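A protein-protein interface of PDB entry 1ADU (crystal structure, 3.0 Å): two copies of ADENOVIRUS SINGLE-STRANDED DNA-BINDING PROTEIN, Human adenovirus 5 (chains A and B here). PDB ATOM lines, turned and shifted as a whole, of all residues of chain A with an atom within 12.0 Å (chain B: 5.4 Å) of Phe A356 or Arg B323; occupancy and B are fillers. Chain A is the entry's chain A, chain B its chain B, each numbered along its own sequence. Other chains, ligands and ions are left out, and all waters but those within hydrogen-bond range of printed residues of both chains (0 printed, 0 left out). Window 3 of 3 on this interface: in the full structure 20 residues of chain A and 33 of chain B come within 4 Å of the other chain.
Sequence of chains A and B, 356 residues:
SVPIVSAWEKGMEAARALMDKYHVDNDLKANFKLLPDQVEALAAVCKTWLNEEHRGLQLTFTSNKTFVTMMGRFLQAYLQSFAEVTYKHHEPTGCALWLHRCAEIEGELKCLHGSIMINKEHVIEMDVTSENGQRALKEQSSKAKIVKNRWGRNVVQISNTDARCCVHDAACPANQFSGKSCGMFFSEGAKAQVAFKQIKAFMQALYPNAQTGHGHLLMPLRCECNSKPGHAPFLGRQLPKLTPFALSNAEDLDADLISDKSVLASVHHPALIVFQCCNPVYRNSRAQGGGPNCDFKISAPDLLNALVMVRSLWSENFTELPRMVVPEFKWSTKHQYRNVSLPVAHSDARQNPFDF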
ATOM      1  N   ARG A 350     -10.886  11.340 -19.857  1.00  0.00           N
ATOM      2  CA  ARG A 350     -11.424   9.987 -19.730  1.00  0.00           C
ATOM      3  C   ARG A 350     -12.425   9.808 -20.851  1.00  0.00           C
ATOM      4  O   ARG A 350     -13.230  10.700 -21.099  1.00  0.00           O
ATOM      5  CB  ARG A 350     -12.161   9.815 -18.401  1.00  0.00           C
ATOM      6  CG  ARG A 350     -11.281   9.709 -17.173  1.00  0.00           C
ATOM      7  CD  ARG A 350     -12.129   9.698 -15.911  1.00  0.00           C
ATOM      8  NE  ARG A 350     -13.183   8.694 -15.991  1.00  0.00           N
ATOM      9  CZ  ARG A 350     -13.082   7.464 -15.499  1.00  0.00           C
ATOM     10  NH1 ARG A 350     -11.971   7.089 -14.876  1.00  0.00           N
ATOM     11  NH2 ARG A 350     -14.072   6.595 -15.675  1.00  0.00           N
ATOM     12  N   GLN A 351     -12.359   8.677 -21.543  1.00  0.00           N
ATOM     13  CA  GLN A 351     -13.291   8.413 -22.631  1.00  0.00           C
ATOM     14  C   GLN A 351     -14.681   8.222 -22.029  1.00  0.00           C
ATOM     15  O   GLN A 351     -15.617   8.946 -22.361  1.00  0.00           O
ATOM     16  CB  GLN A 351     -12.885   7.161 -23.422  1.00  0.00           C
ATOM     17  CG  GLN A 351     -11.582   7.280 -24.223  1.00  0.00           C
ATOM     18  CD  GLN A 351     -10.329   7.227 -23.353  1.00  0.00           C
ATOM     19  OE1 GLN A 351     -10.353   6.699 -22.240  1.00  0.00           O
ATOM     20  NE2 GLN A 351      -9.226   7.772 -23.862  1.00  0.00           N
ATOM     21  N   ASN A 352     -14.787   7.268 -21.106  1.00  0.00           N
ATOM     22  CA  ASN A 352     -16.053   6.958 -20.436  1.00  0.00           C
ATOM     23  C   ASN A 352     -16.290   7.840 -19.211  1.00  0.00           C
ATOM     24  O   ASN A 352     -15.373   8.085 -18.426  1.00  0.00           O
ATOM     25  CB  ASN A 352     -16.083   5.486 -20.019  1.00  0.00           C
ATOM     26  CG  ASN A 352     -16.137   4.545 -21.206  1.00  0.00           C
ATOM     27  OD1 ASN A 352     -17.002   4.667 -22.074  1.00  0.00           O
ATOM     28  ND2 ASN A 352     -15.217   3.588 -21.243  1.00  0.00           N
ATOM     29  N   PRO A 353     -17.530   8.320 -19.025  1.00  0.00           N
ATOM     30  CA  PRO A 353     -17.881   9.178 -17.887  1.00  0.00           C
ATOM     31  C   PRO A 353     -17.969   8.492 -16.524  1.00  0.00           C
ATOM     32  O   PRO A 353     -17.633   9.096 -15.506  1.00  0.00           O
ATOM     33  CB  PRO A 353     -19.234   9.757 -18.303  1.00  0.00           C
ATOM     34  CG  PRO A 353     -19.820   8.685 -19.149  1.00  0.00           C
ATOM     35  CD  PRO A 353     -18.648   8.232 -19.980  1.00  0.00           C
ATOM     36  N   PHE A 354     -18.426   7.241 -16.503  1.00  0.00           N
ATOM     37  CA  PHE A 354     -18.583   6.508 -15.248  1.00  0.00           C
ATOM     38  C   PHE A 354     -17.872   5.163 -15.270  1.00  0.00           C
ATOM     39  O   PHE A 354     -17.877   4.468 -16.288  1.00  0.00           O
ATOM     40  CB  PHE A 354     -20.071   6.255 -14.960  1.00  0.00           C
ATOM     41  CG  PHE A 354     -20.914   7.501 -14.925  1.00  0.00           C
ATOM     42  CD1 PHE A 354     -20.724   8.461 -13.938  1.00  0.00           C
ATOM     43  CD2 PHE A 354     -21.904   7.707 -15.873  1.00  0.00           C
ATOM     44  CE1 PHE A 354     -21.504   9.601 -13.901  1.00  0.00           C
ATOM     45  CE2 PHE A 354     -22.687   8.846 -15.842  1.00  0.00           C
ATOM     46  CZ  PHE A 354     -22.488   9.792 -14.855  1.00  0.00           C
ATOM     47  N   ASP A 355     -17.291   4.793 -14.131  1.00  0.00           N
ATOM     48  CA  ASP A 355     -16.594   3.517 -13.990  1.00  0.00           C
ATOM     49  C   ASP A 355     -17.588   2.443 -13.575  1.00  0.00           C
ATOM     50  O   ASP A 355     -18.128   2.488 -12.469  1.00  0.00           O
ATOM     51  CB  ASP A 355     -15.487   3.607 -12.932  1.00  0.00           C
ATOM     52  CG  ASP A 355     -14.250   4.332 -13.433  1.00  0.00           C
ATOM     53  OD1 ASP A 355     -13.607   3.826 -14.376  1.00  0.00           O
ATOM     54  OD2 ASP A 355     -13.911   5.398 -12.875  1.00  0.00           O
ATOM     55  N   PHE A 356     -17.859   1.516 -14.485  1.00  0.00           N
ATOM     56  CA  PHE A 356     -18.779   0.417 -14.217  1.00  0.00           C
ATOM     57  C   PHE A 356     -17.970  -0.822 -13.833  1.00  0.00           C
ATOM     58  O   PHE A 356     -18.409  -1.557 -12.923  1.00  0.00           O
ATOM     59  CB  PHE A 356     -19.643   0.116 -15.449  1.00  0.00           C
ATOM     60  CG  PHE A 356     -20.630   1.203 -15.789  1.00  0.00           C
ATOM     61  CD1 PHE A 356     -21.751   1.419 -14.993  1.00  0.00           C
ATOM     62  CD2 PHE A 356     -20.446   2.000 -16.912  1.00  0.00           C
ATOM     63  CE1 PHE A 356     -22.677   2.412 -15.317  1.00  0.00           C
ATOM     64  CE2 PHE A 356     -21.367   2.993 -17.240  1.00  0.00           C
ATOM     65  CZ  PHE A 356     -22.482   3.199 -16.440  1.00  0.00           C
ATOM     66  OXT PHE A 356     -16.899  -1.038 -14.444  1.00  0.00           O
ATOM     67  N   SER B  81     -11.356   4.605  -1.956  1.00  0.00           N
ATOM     68  CA  SER B  81     -11.037   3.703  -3.068  1.00  0.00           C
ATOM     69  C   SER B  81      -9.524   3.571  -3.248  1.00  0.00           C
ATOM     70  O   SER B  81      -9.028   2.543  -3.714  1.00  0.00           O
ATOM     71  CB  SER B  81     -11.666   4.213  -4.372  1.00  0.00           C
ATOM     72  OG  SER B  81     -13.079   4.334  -4.264  1.00  0.00           O
ATOM     73  N   LEU B  97     -26.482   6.046 -10.232  1.00  0.00           N
ATOM     74  CA  LEU B  97     -26.619   6.200 -11.675  1.00  0.00           C
ATOM     75  C   LEU B  97     -27.957   5.695 -12.197  1.00  0.00           C
ATOM     76  O   LEU B  97     -28.118   4.501 -12.470  1.00  0.00           O
ATOM     77  CB  LEU B  97     -25.481   5.460 -12.386  1.00  0.00           C
ATOM     78  CG  LEU B  97     -24.248   6.243 -12.855  1.00  0.00           C
ATOM     79  CD1 LEU B  97     -23.810   7.227 -11.813  1.00  0.00           C
ATOM     80  CD2 LEU B  97     -23.127   5.280 -13.174  1.00  0.00           C
ATOM     81  N   THR B 212     -20.475   3.860 -22.827  1.00  0.00           N
ATOM     82  CA  THR B 212     -21.749   4.039 -22.143  1.00  0.00           C
ATOM     83  C   THR B 212     -21.705   5.298 -21.294  1.00  0.00           C
ATOM     84  O   THR B 212     -20.691   5.998 -21.260  1.00  0.00           O
ATOM     85  CB  THR B 212     -22.054   2.841 -21.220  1.00  0.00           C
ATOM     86  OG1 THR B 212     -20.824   2.272 -20.747  1.00  0.00           O
ATOM     87  CG2 THR B 212     -22.872   1.787 -21.951  1.00  0.00           C
ATOM     88  N   GLY B 213     -22.813   5.594 -20.620  1.00  0.00           N
ATOM     89  CA  GLY B 213     -22.858   6.763 -19.762  1.00  0.00           C
ATOM     90  C   GLY B 213     -23.848   7.832 -20.164  1.00  0.00           C
ATOM     91  O   GLY B 213     -24.447   8.461 -19.298  1.00  0.00           O
ATOM     92  N   HIS B 216     -27.355   7.249 -18.615  1.00  0.00           N
ATOM     93  CA  HIS B 216     -27.500   7.327 -17.166  1.00  0.00           C
ATOM     94  C   HIS B 216     -27.607   8.767 -16.689  1.00  0.00           C
ATOM     95  O   HIS B 216     -27.436   9.706 -17.468  1.00  0.00           O
ATOM     96  CB  HIS B 216     -26.319   6.648 -16.471  1.00  0.00           C
ATOM     97  CG  HIS B 216     -26.284   5.162 -16.653  1.00  0.00           C
ATOM     98  ND1 HIS B 216     -26.350   4.280 -15.594  1.00  0.00           N
ATOM     99  CD2 HIS B 216     -26.191   4.402 -17.769  1.00  0.00           C
ATOM    100  CE1 HIS B 216     -26.303   3.041 -16.048  1.00  0.00           C
ATOM    101  NE2 HIS B 216     -26.206   3.087 -17.365  1.00  0.00           N
ATOM    102  N   LEU B 321      -5.819   7.932 -10.897  1.00  0.00           N
ATOM    103  CA  LEU B 321      -7.134   7.959 -10.263  1.00  0.00           C
ATOM    104  C   LEU B 321      -7.541   6.529  -9.949  1.00  0.00           C
ATOM    105  O   LEU B 321      -7.707   5.715 -10.860  1.00  0.00           O
ATOM    106  CB  LEU B 321      -8.182   8.576 -11.195  1.00  0.00           C
ATOM    107  CG  LEU B 321      -8.581  10.048 -11.045  1.00  0.00           C
ATOM    108  CD1 LEU B 321      -9.438  10.470 -12.223  1.00  0.00           C
ATOM    109  CD2 LEU B 321      -9.334  10.261  -9.746  1.00  0.00           C
ATOM    110  N   PRO B 322      -7.676   6.193  -8.658  1.00  0.00           N
ATOM    111  CA  PRO B 322      -8.069   4.840  -8.261  1.00  0.00           C
ATOM    112  C   PRO B 322      -9.472   4.523  -8.755  1.00  0.00           C
ATOM    113  O   PRO B 322     -10.204   5.416  -9.183  1.00  0.00           O
ATOM    114  CB  PRO B 322      -8.019   4.910  -6.736  1.00  0.00           C
ATOM    115  CG  PRO B 322      -8.358   6.334  -6.460  1.00  0.00           C
ATOM    116  CD  PRO B 322      -7.518   7.054  -7.478  1.00  0.00           C
ATOM    117  N   ARG B 323      -9.835   3.247  -8.710  1.00  0.00           N
ATOM    118  CA  ARG B 323     -11.156   2.820  -9.151  1.00  0.00           C
ATOM    119  C   ARG B 323     -12.201   3.221  -8.112  1.00  0.00           C
ATOM    120  O   ARG B 323     -12.115   2.833  -6.944  1.00  0.00           O
ATOM    121  CB  ARG B 323     -11.188   1.309  -9.364  1.00  0.00           C
ATOM    122  CG  ARG B 323     -12.535   0.785  -9.809  1.00  0.00           C
ATOM    123  CD  ARG B 323     -12.550  -0.726  -9.818  1.00  0.00           C
ATOM    124  NE  ARG B 323     -13.834  -1.243 -10.275  1.00  0.00           N
ATOM    125  CZ  ARG B 323     -14.265  -1.174 -11.531  1.00  0.00           C
ATOM    126  NH1 ARG B 323     -13.515  -0.609 -12.471  1.00  0.00           N
ATOM    127  NH2 ARG B 323     -15.454  -1.669 -11.846  1.00  0.00           N
ATOM    128  N   MET B 324     -13.172   4.017  -8.538  1.00  0.00           N
ATOM    129  CA  MET B 324     -14.237   4.469  -7.664  1.00  0.00           C
ATOM    130  C   MET B 324     -15.529   4.303  -8.442  1.00  0.00           C
ATOM    131  O   MET B 324     -15.765   4.998  -9.436  1.00  0.00           O
ATOM    132  CB  MET B 324     -14.014   5.929  -7.276  1.00  0.00           C
ATOM    133  CG  MET B 324     -15.071   6.514  -6.351  1.00  0.00           C
ATOM    134  SD  MET B 324     -16.610   6.958  -7.189  1.00  0.00           S
ATOM    135  CE  MET B 324     -16.391   8.721  -7.409  1.00  0.00           C
ATOM    136  N   VAL B 325     -16.329   3.328  -8.020  1.00  0.00           N
ATOM    137  CA  VAL B 325     -17.597   3.034  -8.673  1.00  0.00           C
ATOM    138  C   VAL B 325     -18.776   3.638  -7.929  1.00  0.00           C
ATOM    139  O   VAL B 325     -18.869   3.552  -6.700  1.00  0.00           O
ATOM    140  CB  VAL B 325     -17.823   1.507  -8.809  1.00  0.00           C
ATOM    141  CG1 VAL B 325     -19.156   1.220  -9.506  1.00  0.00           C
ATOM    142  CG2 VAL B 325     -16.674   0.875  -9.580  1.00  0.00           C
ATOM    143  N   GLU B 328     -25.360   1.731  -9.524  1.00  0.00           N
ATOM    144  CA  GLU B 328     -26.367   1.901 -10.561  1.00  0.00           C
ATOM    145  C   GLU B 328     -27.700   1.787  -9.830  1.00  0.00           C
ATOM    146  O   GLU B 328     -27.930   0.827  -9.096  1.00  0.00           O
ATOM    147  CB  GLU B 328     -26.246   0.825 -11.639  1.00  0.00           C
ATOM    148  CG  GLU B 328     -27.119   1.104 -12.859  1.00  0.00           C
ATOM    149  CD  GLU B 328     -26.702   0.305 -14.080  1.00  0.00           C
ATOM    150  OE1 GLU B 328     -25.504   0.327 -14.435  1.00  0.00           O
ATOM    151  OE2 GLU B 328     -27.576  -0.334 -14.697  1.00  0.00           O
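Among the printed residues, merely in contact across the chains: Pro A353 with Thr B212 (3.3 Å), Asp A355 with Val B325 (3.4 Å), Phe A354 with Leu B97 (3.6 Å), Phe A356 with Leu B97 (3.6 Å), Phe A356 with Thr B212 (3.6 Å), Phe A356 with Glu B328 (3.6 Å), Asn A352 with Thr B212 (3.6 Å), Pro A353 with Gly B213 (3.6 Å), Phe A356 with His B216 (3.8 Å), Asp A355 with Met B324 (3.8 Å) and Phe A354 with Gly B213 (3.9 Å).
Of the printed residues of chain B, Phe A356 touches Leu B97 (3.6 Å), Thr B212 (3.6 Å), His B216 (3.8 Å), Arg B323 (3.0 Å) and Glu B328 (3.6 Å). Arg B323 touches one residue of chain A. No residue of chain A comes within 4 Å of Ser B81. Of chain A, only Phe A354 (3.6 Å) and Phe A356 (3.6 Å) come within 4 Å of Leu B97. Thr B212 touches just these residues of chain A: Asn A352 (3.6 Å), Pro A353 (3.3 Å) and Phe A356 (3.6 Å). Of the printed residues of chain A, Gly B213 touches Pro A353 and Phe A354. Pro B322 touches none of the printed residues of chain A. Of chain A, only Asp A355 comes within 4 Å of Val B325. Of the printed residues of chain A, His B216 touches Phe A356 (3.8 Å). Printed residues of chain B within 4 Å of Phe A354: Leu B97 and Gly B213. Printed residues of chain B within 4 Å of Asn A352: Thr B212. Of the printed residues of chain A, Glu B328 touches Phe A356 (3.6 Å). Printed residues of chain B within 4 Å of Pro A353: Thr B212 (3.3 Å) and Gly B213 (3.6 Å). The nearest residue of chain B that does not touch Phe A356 is Val B325 (4.5 Å). The nearest residue of chain A that does not touch Arg B323 is Asp A355 (4.7 Å).
The guanidinium group (NE) of Arg A350 sits at hydrogen-bond distance from the backbone carbonyl oxygen (O) of Asn A352 (3.3 Å). OD2 of Asp A355 lies within salt-bridge range of NH2 of Arg A350, at 3.0 Å. The side-chain hydroxyl (OG) of Ser B81 lies close to the backbone carbonyl oxygen (O) of Arg B323 (3.2 Å).
No position is printed for both chains. Of the 12 pairs that touch across the chains among the printed residues, none has its exchanged pair printed and touching as well.
The chain-end carboxylate of Phe A356 is in salt-bridge range of the guanidinium group of Arg B323 (3.0 Å).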
